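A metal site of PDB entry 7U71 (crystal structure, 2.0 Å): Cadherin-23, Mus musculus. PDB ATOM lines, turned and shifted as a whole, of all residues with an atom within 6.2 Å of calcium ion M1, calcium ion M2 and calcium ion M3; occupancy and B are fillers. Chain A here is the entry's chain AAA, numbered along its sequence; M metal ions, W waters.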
ATOM      1  N   GLU A 124       7.805 -18.806 -25.536  1.00  0.00           N
ATOM      2  CA  GLU A 124       8.104 -19.994 -26.363  1.00  0.00           C
ATOM      3  C   GLU A 124       6.910 -20.951 -26.302  1.00  0.00           C
ATOM      4  O   GLU A 124       6.842 -21.822 -27.161  1.00  0.00           O
ATOM      5  CB  GLU A 124       9.418 -20.657 -25.907  1.00  0.00           C
ATOM      6  CG  GLU A 124       9.487 -21.053 -24.447  1.00  0.00           C
ATOM      7  CD  GLU A 124      10.619 -22.015 -24.112  1.00  0.00           C
ATOM      8  OE1 GLU A 124      10.985 -22.877 -24.989  1.00  0.00           O
ATOM      9  OE2 GLU A 124      11.121 -21.930 -22.967  1.00  0.00           O
ATOM     10  N   LEU A 179       7.266 -23.140 -30.986  1.00  0.00           N
ATOM     11  CA  LEU A 179       8.537 -22.453 -30.709  1.00  0.00           C
ATOM     12  C   LEU A 179       9.279 -23.205 -29.619  1.00  0.00           C
ATOM     13  O   LEU A 179       8.662 -23.950 -28.865  1.00  0.00           O
ATOM     14  CB  LEU A 179       8.286 -20.992 -30.332  1.00  0.00           C
ATOM     15  CG  LEU A 179       7.361 -20.220 -31.274  1.00  0.00           C
ATOM     16  CD1 LEU A 179       6.966 -18.890 -30.674  1.00  0.00           C
ATOM     17  CD2 LEU A 179       7.985 -20.042 -32.643  1.00  0.00           C
ATOM     18  N   ASP A 180      10.581 -22.930 -29.504  1.00  0.00           N
ATOM     19  CA  ASP A 180      11.420 -23.516 -28.442  1.00  0.00           C
ATOM     20  C   ASP A 180      12.601 -22.577 -28.244  1.00  0.00           C
ATOM     21  O   ASP A 180      13.543 -22.667 -29.071  1.00  0.00           O
ATOM     22  CB  ASP A 180      11.879 -24.928 -28.844  1.00  0.00           C
ATOM     23  CG  ASP A 180      12.757 -25.545 -27.772  1.00  0.00           C
ATOM     24  OD1 ASP A 180      12.813 -25.017 -26.620  1.00  0.00           O
ATOM     25  OD2 ASP A 180      13.348 -26.577 -28.067  1.00  0.00           O
ATOM     26  N   ARG A 181      12.607 -21.793 -27.157  1.00  0.00           N
ATOM     27  CA  ARG A 181      13.710 -20.845 -26.830  1.00  0.00           C
ATOM     28  C   ARG A 181      15.047 -21.598 -26.725  1.00  0.00           C
ATOM     29  O   ARG A 181      16.092 -21.006 -27.100  1.00  0.00           O
ATOM     30  CB  ARG A 181      13.453 -20.111 -25.518  1.00  0.00           C
ATOM     31  CG  ARG A 181      14.422 -18.965 -25.229  1.00  0.00           C
ATOM     32  CD  ARG A 181      14.704 -18.719 -23.766  1.00  0.00           C
ATOM     33  NE  ARG A 181      15.362 -19.875 -23.198  1.00  0.00           N
ATOM     34  CZ  ARG A 181      16.647 -20.206 -23.351  1.00  0.00           C
ATOM     35  NH1 ARG A 181      17.483 -19.414 -23.996  1.00  0.00           N
ATOM     36  NH2 ARG A 181      17.071 -21.345 -22.841  1.00  0.00           N
ATOM     37  N   GLU A 182      15.025 -22.842 -26.253  1.00  0.00           N
ATOM     38  CA  GLU A 182      16.276 -23.660 -26.074  1.00  0.00           C
ATOM     39  C   GLU A 182      16.865 -24.054 -27.441  1.00  0.00           C
ATOM     40  O   GLU A 182      18.039 -24.443 -27.465  1.00  0.00           O
ATOM     41  CB  GLU A 182      16.009 -24.914 -25.237  1.00  0.00           C
ATOM     42  CG  GLU A 182      15.968 -24.624 -23.756  1.00  0.00           C
ATOM     43  CD  GLU A 182      14.751 -23.894 -23.218  1.00  0.00           C
ATOM     44  OE1 GLU A 182      14.942 -22.933 -22.457  1.00  0.00           O
ATOM     45  OE2 GLU A 182      13.607 -24.265 -23.616  1.00  0.00           O
ATOM     46  N   GLU A 183      16.096 -23.994 -28.529  1.00  0.00           N
ATOM     47  CA  GLU A 183      16.590 -24.256 -29.900  1.00  0.00           C
ATOM     48  C   GLU A 183      16.938 -22.911 -30.546  1.00  0.00           C
ATOM     49  O   GLU A 183      18.063 -22.782 -31.045  1.00  0.00           O
ATOM     50  CB  GLU A 183      15.632 -25.142 -30.698  1.00  0.00           C
ATOM     51  CG  GLU A 183      16.031 -25.281 -32.168  1.00  0.00           C
ATOM     52  CD  GLU A 183      17.406 -25.868 -32.488  1.00  0.00           C
ATOM     53  OE1 GLU A 183      17.868 -26.728 -31.711  1.00  0.00           O
ATOM     54  OE2 GLU A 183      18.029 -25.448 -33.533  1.00  0.00           O
ATOM     55  N   LEU A 212      10.731 -15.495 -25.418  1.00  0.00           N
ATOM     56  CA  LEU A 212      10.848 -15.494 -23.936  1.00  0.00           C
ATOM     57  C   LEU A 212      10.815 -16.908 -23.385  1.00  0.00           C
ATOM     58  O   LEU A 212      10.080 -17.793 -23.921  1.00  0.00           O
ATOM     59  CB  LEU A 212       9.752 -14.629 -23.309  1.00  0.00           C
ATOM     60  CG  LEU A 212       9.677 -13.242 -23.950  1.00  0.00           C
ATOM     61  CD1 LEU A 212       8.375 -12.561 -23.605  1.00  0.00           C
ATOM     62  CD2 LEU A 212      10.904 -12.436 -23.554  1.00  0.00           C
ATOM     63  N   ASP A 213      11.556 -17.084 -22.283  1.00  0.00           N
ATOM     64  CA  ASP A 213      11.706 -18.420 -21.666  1.00  0.00           C
ATOM     65  C   ASP A 213      10.440 -18.808 -20.924  1.00  0.00           C
ATOM     66  O   ASP A 213       9.851 -17.981 -20.262  1.00  0.00           O
ATOM     67  CB  ASP A 213      12.911 -18.466 -20.724  1.00  0.00           C
ATOM     68  CG  ASP A 213      13.308 -19.866 -20.310  1.00  0.00           C
ATOM     69  OD1 ASP A 213      13.350 -20.748 -21.197  1.00  0.00           O
ATOM     70  OD2 ASP A 213      13.554 -20.048 -19.074  1.00  0.00           O
ATOM     71  N   VAL A 214      10.094 -20.083 -21.009  1.00  0.00           N
ATOM     72  CA  VAL A 214       9.132 -20.763 -20.109  1.00  0.00           C
ATOM     73  C   VAL A 214       9.934 -21.821 -19.346  1.00  0.00           C
ATOM     74  O   VAL A 214      10.931 -22.347 -19.890  1.00  0.00           O
ATOM     75  CB  VAL A 214       7.990 -21.363 -20.947  1.00  0.00           C
ATOM     76  CG1 VAL A 214       7.130 -22.289 -20.113  1.00  0.00           C
ATOM     77  CG2 VAL A 214       7.172 -20.211 -21.576  1.00  0.00           C
ATOM     78  N   ASN A 215       9.495 -22.140 -18.118  1.00  0.00           N
ATOM     79  CA  ASN A 215      10.137 -23.200 -17.310  1.00  0.00           C
ATOM     80  C   ASN A 215       9.670 -24.541 -17.844  1.00  0.00           C
ATOM     81  O   ASN A 215       8.745 -25.138 -17.268  1.00  0.00           O
ATOM     82  CB  ASN A 215       9.830 -23.094 -15.821  1.00  0.00           C
ATOM     83  CG  ASN A 215      10.788 -23.951 -15.026  1.00  0.00           C
ATOM     84  OD1 ASN A 215      11.923 -24.218 -15.465  1.00  0.00           O
ATOM     85  ND2 ASN A 215      10.341 -24.414 -13.867  1.00  0.00           N
ATOM     86  N   ASP A 216      10.326 -25.049 -18.884  1.00  0.00           N
ATOM     87  CA  ASP A 216       9.856 -26.306 -19.510  1.00  0.00           C
ATOM     88  C   ASP A 216      10.956 -27.378 -19.513  1.00  0.00           C
ATOM     89  O   ASP A 216      10.729 -28.377 -20.193  1.00  0.00           O
ATOM     90  CB  ASP A 216       9.289 -26.004 -20.898  1.00  0.00           C
ATOM     91  CG  ASP A 216      10.233 -25.343 -21.903  1.00  0.00           C
ATOM     92  OD1 ASP A 216      11.325 -24.936 -21.535  1.00  0.00           O
ATOM     93  OD2 ASP A 216       9.871 -25.335 -23.065  1.00  0.00           O
ATOM     94  N   ASN A 217      12.069 -27.154 -18.802  1.00  0.00           N
ATOM     95  CA  ASN A 217      13.153 -28.152 -18.602  1.00  0.00           C
ATOM     96  C   ASN A 217      13.395 -28.394 -17.113  1.00  0.00           C
ATOM     97  O   ASN A 217      13.560 -27.442 -16.322  1.00  0.00           O
ATOM     98  CB  ASN A 217      14.473 -27.772 -19.265  1.00  0.00           C
ATOM     99  CG  ASN A 217      14.342 -27.718 -20.764  1.00  0.00           C
ATOM    100  OD1 ASN A 217      14.556 -28.705 -21.447  1.00  0.00           O
ATOM    101  ND2 ASN A 217      13.901 -26.588 -21.285  1.00  0.00           N
ATOM    102  N   PRO A 218      13.350 -29.676 -16.692  1.00  0.00           N
ATOM    103  CA  PRO A 218      13.592 -30.048 -15.315  1.00  0.00           C
ATOM    104  C   PRO A 218      15.088 -30.013 -15.023  1.00  0.00           C
ATOM    105  O   PRO A 218      15.936 -30.128 -15.908  1.00  0.00           O
ATOM    106  CB  PRO A 218      13.022 -31.465 -15.237  1.00  0.00           C
ATOM    107  CG  PRO A 218      13.269 -32.044 -16.618  1.00  0.00           C
ATOM    108  CD  PRO A 218      13.104 -30.844 -17.541  1.00  0.00           C
ATOM    109  N   PRO A 219      15.464 -29.953 -13.745  1.00  0.00           N
ATOM    110  CA  PRO A 219      16.833 -30.249 -13.357  1.00  0.00           C
ATOM    111  C   PRO A 219      17.164 -31.661 -13.848  1.00  0.00           C
ATOM    112  O   PRO A 219      16.310 -32.506 -13.892  1.00  0.00           O
ATOM    113  CB  PRO A 219      16.851 -30.150 -11.825  1.00  0.00           C
ATOM    114  CG  PRO A 219      15.580 -29.465 -11.450  1.00  0.00           C
ATOM    115  CD  PRO A 219      14.593 -29.700 -12.588  1.00  0.00           C
ATOM    116  N   ASP A 248      20.237 -27.419 -15.819  1.00  0.00           N
ATOM    117  CA  ASP A 248      18.860 -27.068 -16.233  1.00  0.00           C
ATOM    118  C   ASP A 248      18.980 -26.222 -17.490  1.00  0.00           C
ATOM    119  O   ASP A 248      19.694 -25.229 -17.477  1.00  0.00           O
ATOM    120  CB  ASP A 248      18.129 -26.416 -15.081  1.00  0.00           C
ATOM    121  CG  ASP A 248      16.648 -26.179 -15.316  1.00  0.00           C
ATOM    122  OD1 ASP A 248      16.317 -25.689 -16.416  1.00  0.00           O
ATOM    123  OD2 ASP A 248      15.880 -26.359 -14.326  1.00  0.00           O
ATOM    124  N   ARG A 249      18.272 -26.610 -18.538  1.00  0.00           N
ATOM    125  CA  ARG A 249      18.399 -25.992 -19.871  1.00  0.00           C
ATOM    126  C   ARG A 249      17.698 -24.631 -19.966  1.00  0.00           C
ATOM    127  O   ARG A 249      17.870 -23.967 -21.013  1.00  0.00           O
ATOM    128  CB  ARG A 249      17.828 -26.970 -20.907  1.00  0.00           C
ATOM    129  CG  ARG A 249      18.737 -28.175 -21.159  1.00  0.00           C
ATOM    130  CD  ARG A 249      18.195 -29.108 -22.223  1.00  0.00           C
ATOM    131  NE  ARG A 249      18.387 -28.647 -23.593  1.00  0.00           N
ATOM    132  CZ  ARG A 249      17.422 -28.412 -24.488  1.00  0.00           C
ATOM    133  NH1 ARG A 249      16.140 -28.490 -24.152  1.00  0.00           N
ATOM    134  NH2 ARG A 249      17.760 -28.076 -25.718  1.00  0.00           N
ATOM    135  N   ASP A 250      16.921 -24.215 -18.968  1.00  0.00           N
ATOM    136  CA  ASP A 250      16.171 -22.938 -19.061  1.00  0.00           C
ATOM    137  C   ASP A 250      17.144 -21.832 -18.688  1.00  0.00           C
ATOM    138  O   ASP A 250      18.326 -22.119 -18.610  1.00  0.00           O
ATOM    139  CB  ASP A 250      14.899 -22.961 -18.203  1.00  0.00           C
ATOM    140  CG  ASP A 250      13.962 -24.084 -18.589  1.00  0.00           C
ATOM    141  OD1 ASP A 250      13.608 -24.183 -19.785  1.00  0.00           O
ATOM    142  OD2 ASP A 250      13.588 -24.844 -17.713  1.00  0.00           O
ATOM    143  N   ILE A 251      16.667 -20.604 -18.456  1.00  0.00           N
ATOM    144  CA  ILE A 251      17.545 -19.452 -18.127  1.00  0.00           C
ATOM    145  C   ILE A 251      16.949 -18.686 -16.947  1.00  0.00           C
ATOM    146  O   ILE A 251      15.740 -18.928 -16.644  1.00  0.00           O
ATOM    147  CB  ILE A 251      17.738 -18.562 -19.363  1.00  0.00           C
ATOM    148  CG1 ILE A 251      16.393 -18.054 -19.915  1.00  0.00           C
ATOM    149  CG2 ILE A 251      18.580 -19.292 -20.393  1.00  0.00           C
ATOM    150  CD1 ILE A 251      16.532 -16.930 -20.928  1.00  0.00           C
ATOM    151  N   ILE A 253      15.650 -17.447 -13.486  1.00  0.00           N
ATOM    152  CA  ILE A 253      15.142 -18.201 -12.306  1.00  0.00           C
ATOM    153  C   ILE A 253      14.675 -19.602 -12.702  1.00  0.00           C
ATOM    154  O   ILE A 253      14.635 -20.462 -11.794  1.00  0.00           O
ATOM    155  CB  ILE A 253      14.008 -17.506 -11.499  1.00  0.00           C
ATOM    156  CG1 ILE A 253      12.968 -16.816 -12.373  1.00  0.00           C
ATOM    157  CG2 ILE A 253      14.584 -16.570 -10.437  1.00  0.00           C
ATOM    158  CD1 ILE A 253      12.195 -17.734 -13.236  1.00  0.00           C
ATOM    159  N   ASN A 254      14.365 -19.847 -13.983  1.00  0.00           N
ATOM    160  CA  ASN A 254      13.886 -21.173 -14.442  1.00  0.00           C
ATOM    161  C   ASN A 254      15.040 -22.195 -14.353  1.00  0.00           C
ATOM    162  O   ASN A 254      14.761 -23.386 -14.442  1.00  0.00           O
ATOM    163  CB  ASN A 254      13.275 -21.132 -15.845  1.00  0.00           C
ATOM    164  CG  ASN A 254      12.055 -20.230 -15.885  1.00  0.00           C
ATOM    165  OD1 ASN A 254      11.278 -20.171 -14.926  1.00  0.00           O
ATOM    166  ND2 ASN A 254      11.844 -19.565 -17.011  1.00  0.00           N
ATOM    167  N   SER A 255      16.290 -21.761 -14.169  1.00  0.00           N
ATOM    168  CA  SER A 255      17.426 -22.706 -14.052  1.00  0.00           C
ATOM    169  C   SER A 255      18.186 -22.563 -12.740  1.00  0.00           C
ATOM    170  O   SER A 255      19.286 -23.128 -12.664  1.00  0.00           O
ATOM    171  CB  SER A 255      18.329 -22.551 -15.220  1.00  0.00           C
ATOM    172  OG  SER A 255      18.847 -21.253 -15.299  1.00  0.00           O
ATOM    173  N   LEU A 257      18.678 -23.649  -9.095  1.00  0.00           N
ATOM    174  CA  LEU A 257      18.353 -24.957  -8.481  1.00  0.00           C
ATOM    175  C   LEU A 257      18.444 -24.894  -6.954  1.00  0.00           C
ATOM    176  O   LEU A 257      19.375 -24.237  -6.438  1.00  0.00           O
ATOM    177  CB  LEU A 257      19.335 -25.968  -9.043  1.00  0.00           C
ATOM    178  CG  LEU A 257      19.195 -26.172 -10.558  1.00  0.00           C
ATOM    179  CD1 LEU A 257      20.007 -27.384 -11.020  1.00  0.00           C
ATOM    180  CD2 LEU A 257      17.744 -26.326 -10.944  1.00  0.00           C
ATOM    181  N   ASP A 302      13.931 -26.581  -9.449  1.00  0.00           N
ATOM    182  CA  ASP A 302      14.251 -25.251 -10.018  1.00  0.00           C
ATOM    183  C   ASP A 302      13.321 -24.225  -9.367  1.00  0.00           C
ATOM    184  O   ASP A 302      12.403 -24.634  -8.674  1.00  0.00           O
ATOM    185  CB  ASP A 302      14.187 -25.240 -11.550  1.00  0.00           C
ATOM    186  CG  ASP A 302      12.862 -25.621 -12.196  1.00  0.00           C
ATOM    187  OD1 ASP A 302      11.790 -25.485 -11.561  1.00  0.00           O
ATOM    188  OD2 ASP A 302      12.922 -26.045 -13.380  1.00  0.00           O
ATOM    189  N   GLY A 304      11.460 -21.848 -11.107  1.00  0.00           N
ATOM    190  CA  GLY A 304      10.461 -21.355 -12.093  1.00  0.00           C
ATOM    191  C   GLY A 304       9.035 -21.811 -11.788  1.00  0.00           C
ATOM    192  O   GLY A 304       8.811 -22.409 -10.722  1.00  0.00           O
ATOM    193  N   LEU A 308       9.747 -27.532 -11.436  1.00  0.00           N
ATOM    194  CA  LEU A 308      10.129 -28.855 -11.974  1.00  0.00           C
ATOM    195  C   LEU A 308      11.222 -29.425 -11.075  1.00  0.00           C
ATOM    196  O   LEU A 308      12.004 -28.655 -10.527  1.00  0.00           O
ATOM    197  CB  LEU A 308      10.630 -28.676 -13.416  1.00  0.00           C
ATOM    198  CG  LEU A 308       9.576 -28.132 -14.375  1.00  0.00           C
ATOM    199  CD1 LEU A 308      10.163 -27.972 -15.790  1.00  0.00           C
ATOM    200  CD2 LEU A 308       8.355 -29.035 -14.363  1.00  0.00           C
HETATM  201 CA    CA M   1      12.610 -22.866 -21.483  1.00  0.00          CA
HETATM  202 CA    CA M   2      11.678 -25.036 -24.629  1.00  0.00          CA
HETATM  203 CA    CA M   3      13.972 -25.409 -15.407  1.00  0.00          CA
HETATM  204  O   HOH W   1      12.400 -27.267 -24.068  1.00  0.00           O
HETATM  205  O   HOH W   2       9.859 -25.961 -26.014  1.00  0.00           O
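Within 4 Å of calcium ion M2: Glu 124, Asp 180, Glu 182 and Asp 216. The nearest printed residue that does not touch calcium ion M2 is Arg 181 (4.2 Å).
Calcium ion M3 is bound by O of Asn 217 (2.3 Å), OD2 of Asp 302 (2.4 Å), OD1 of Asn 215 (2.4 Å), O of Asn 254 (2.4 Å), OD2 of Asp 248 (2.4 Å), OD2 of Asp 250 (2.4 Å) and OD1 of Asp 248 (2.6 Å). Calcium ion M3 has seven donor atoms within binding distance.
Of the 25 residues printed, 6 come within 4 Å of calcium ion M3.
Calcium ion M2 is bound by the side-chain carboxylate of Asp 180, the side-chain carboxylate of Glu 124, the side-chain carboxylate of Glu 182, the side-chain carboxylate of Asp 216, water W1 and water W2. Slightly farther from calcium ion M2 lies the side-chain carboxylate (OD1) of Asp 216 (3.1 Å).
Seven residues have an atom within 4 Å of calcium ion M1: Glu 124, Glu 182, Asp 213, Val 214, Asp 216, Asn 217 and Asp 250.
The side-chain carboxylate (OE2) of Glu 182 lies close to the side-chain amide nitrogen (ND2) of Asn 217 (3.3 Å). OD2 of Asp 213 is in hydrogen-bond range of ND2 of Asn 254. The side-chain carboxylate (OD1) of Asp 216 lies close to the side-chain amide nitrogen (ND2) of Asn 217, 3.1 Å away. NH1 of Arg 249 sits at hydrogen-bond distance from OD1 of Asn 217, at 3.1 Å. OE1 of Glu 124 lies close to N of Arg 181 (2.9 Å). OD1 of Asp 302 is in hydrogen-bond range of N of Leu 308, 2.9 Å away. The side-chain carboxylate of Asp 213 lies close to the guanidinium group of Arg 181, 3.0 Å away. NH2 of Arg 181 sits close to OE1 of Glu 182, at 2.7 Å.
Calcium ion M1 is bound by the side-chain carboxylate (OD1) of Asp 213 (2.3 Å), the side-chain carboxylate (OE2) of Glu 124 (2.3 Å), the side-chain carboxylate (OD1) of Asp 250 (2.4 Å), the backbone carbonyl oxygen (O) of Val 214 (2.4 Å), the side-chain carboxylate (OD1) of Asp 216 (2.4 Å), the side-chain carboxylate (OE1) of Glu 182 (2.5 Å) and the side-chain carboxylate (OE2) of Glu 182 (2.7 Å).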
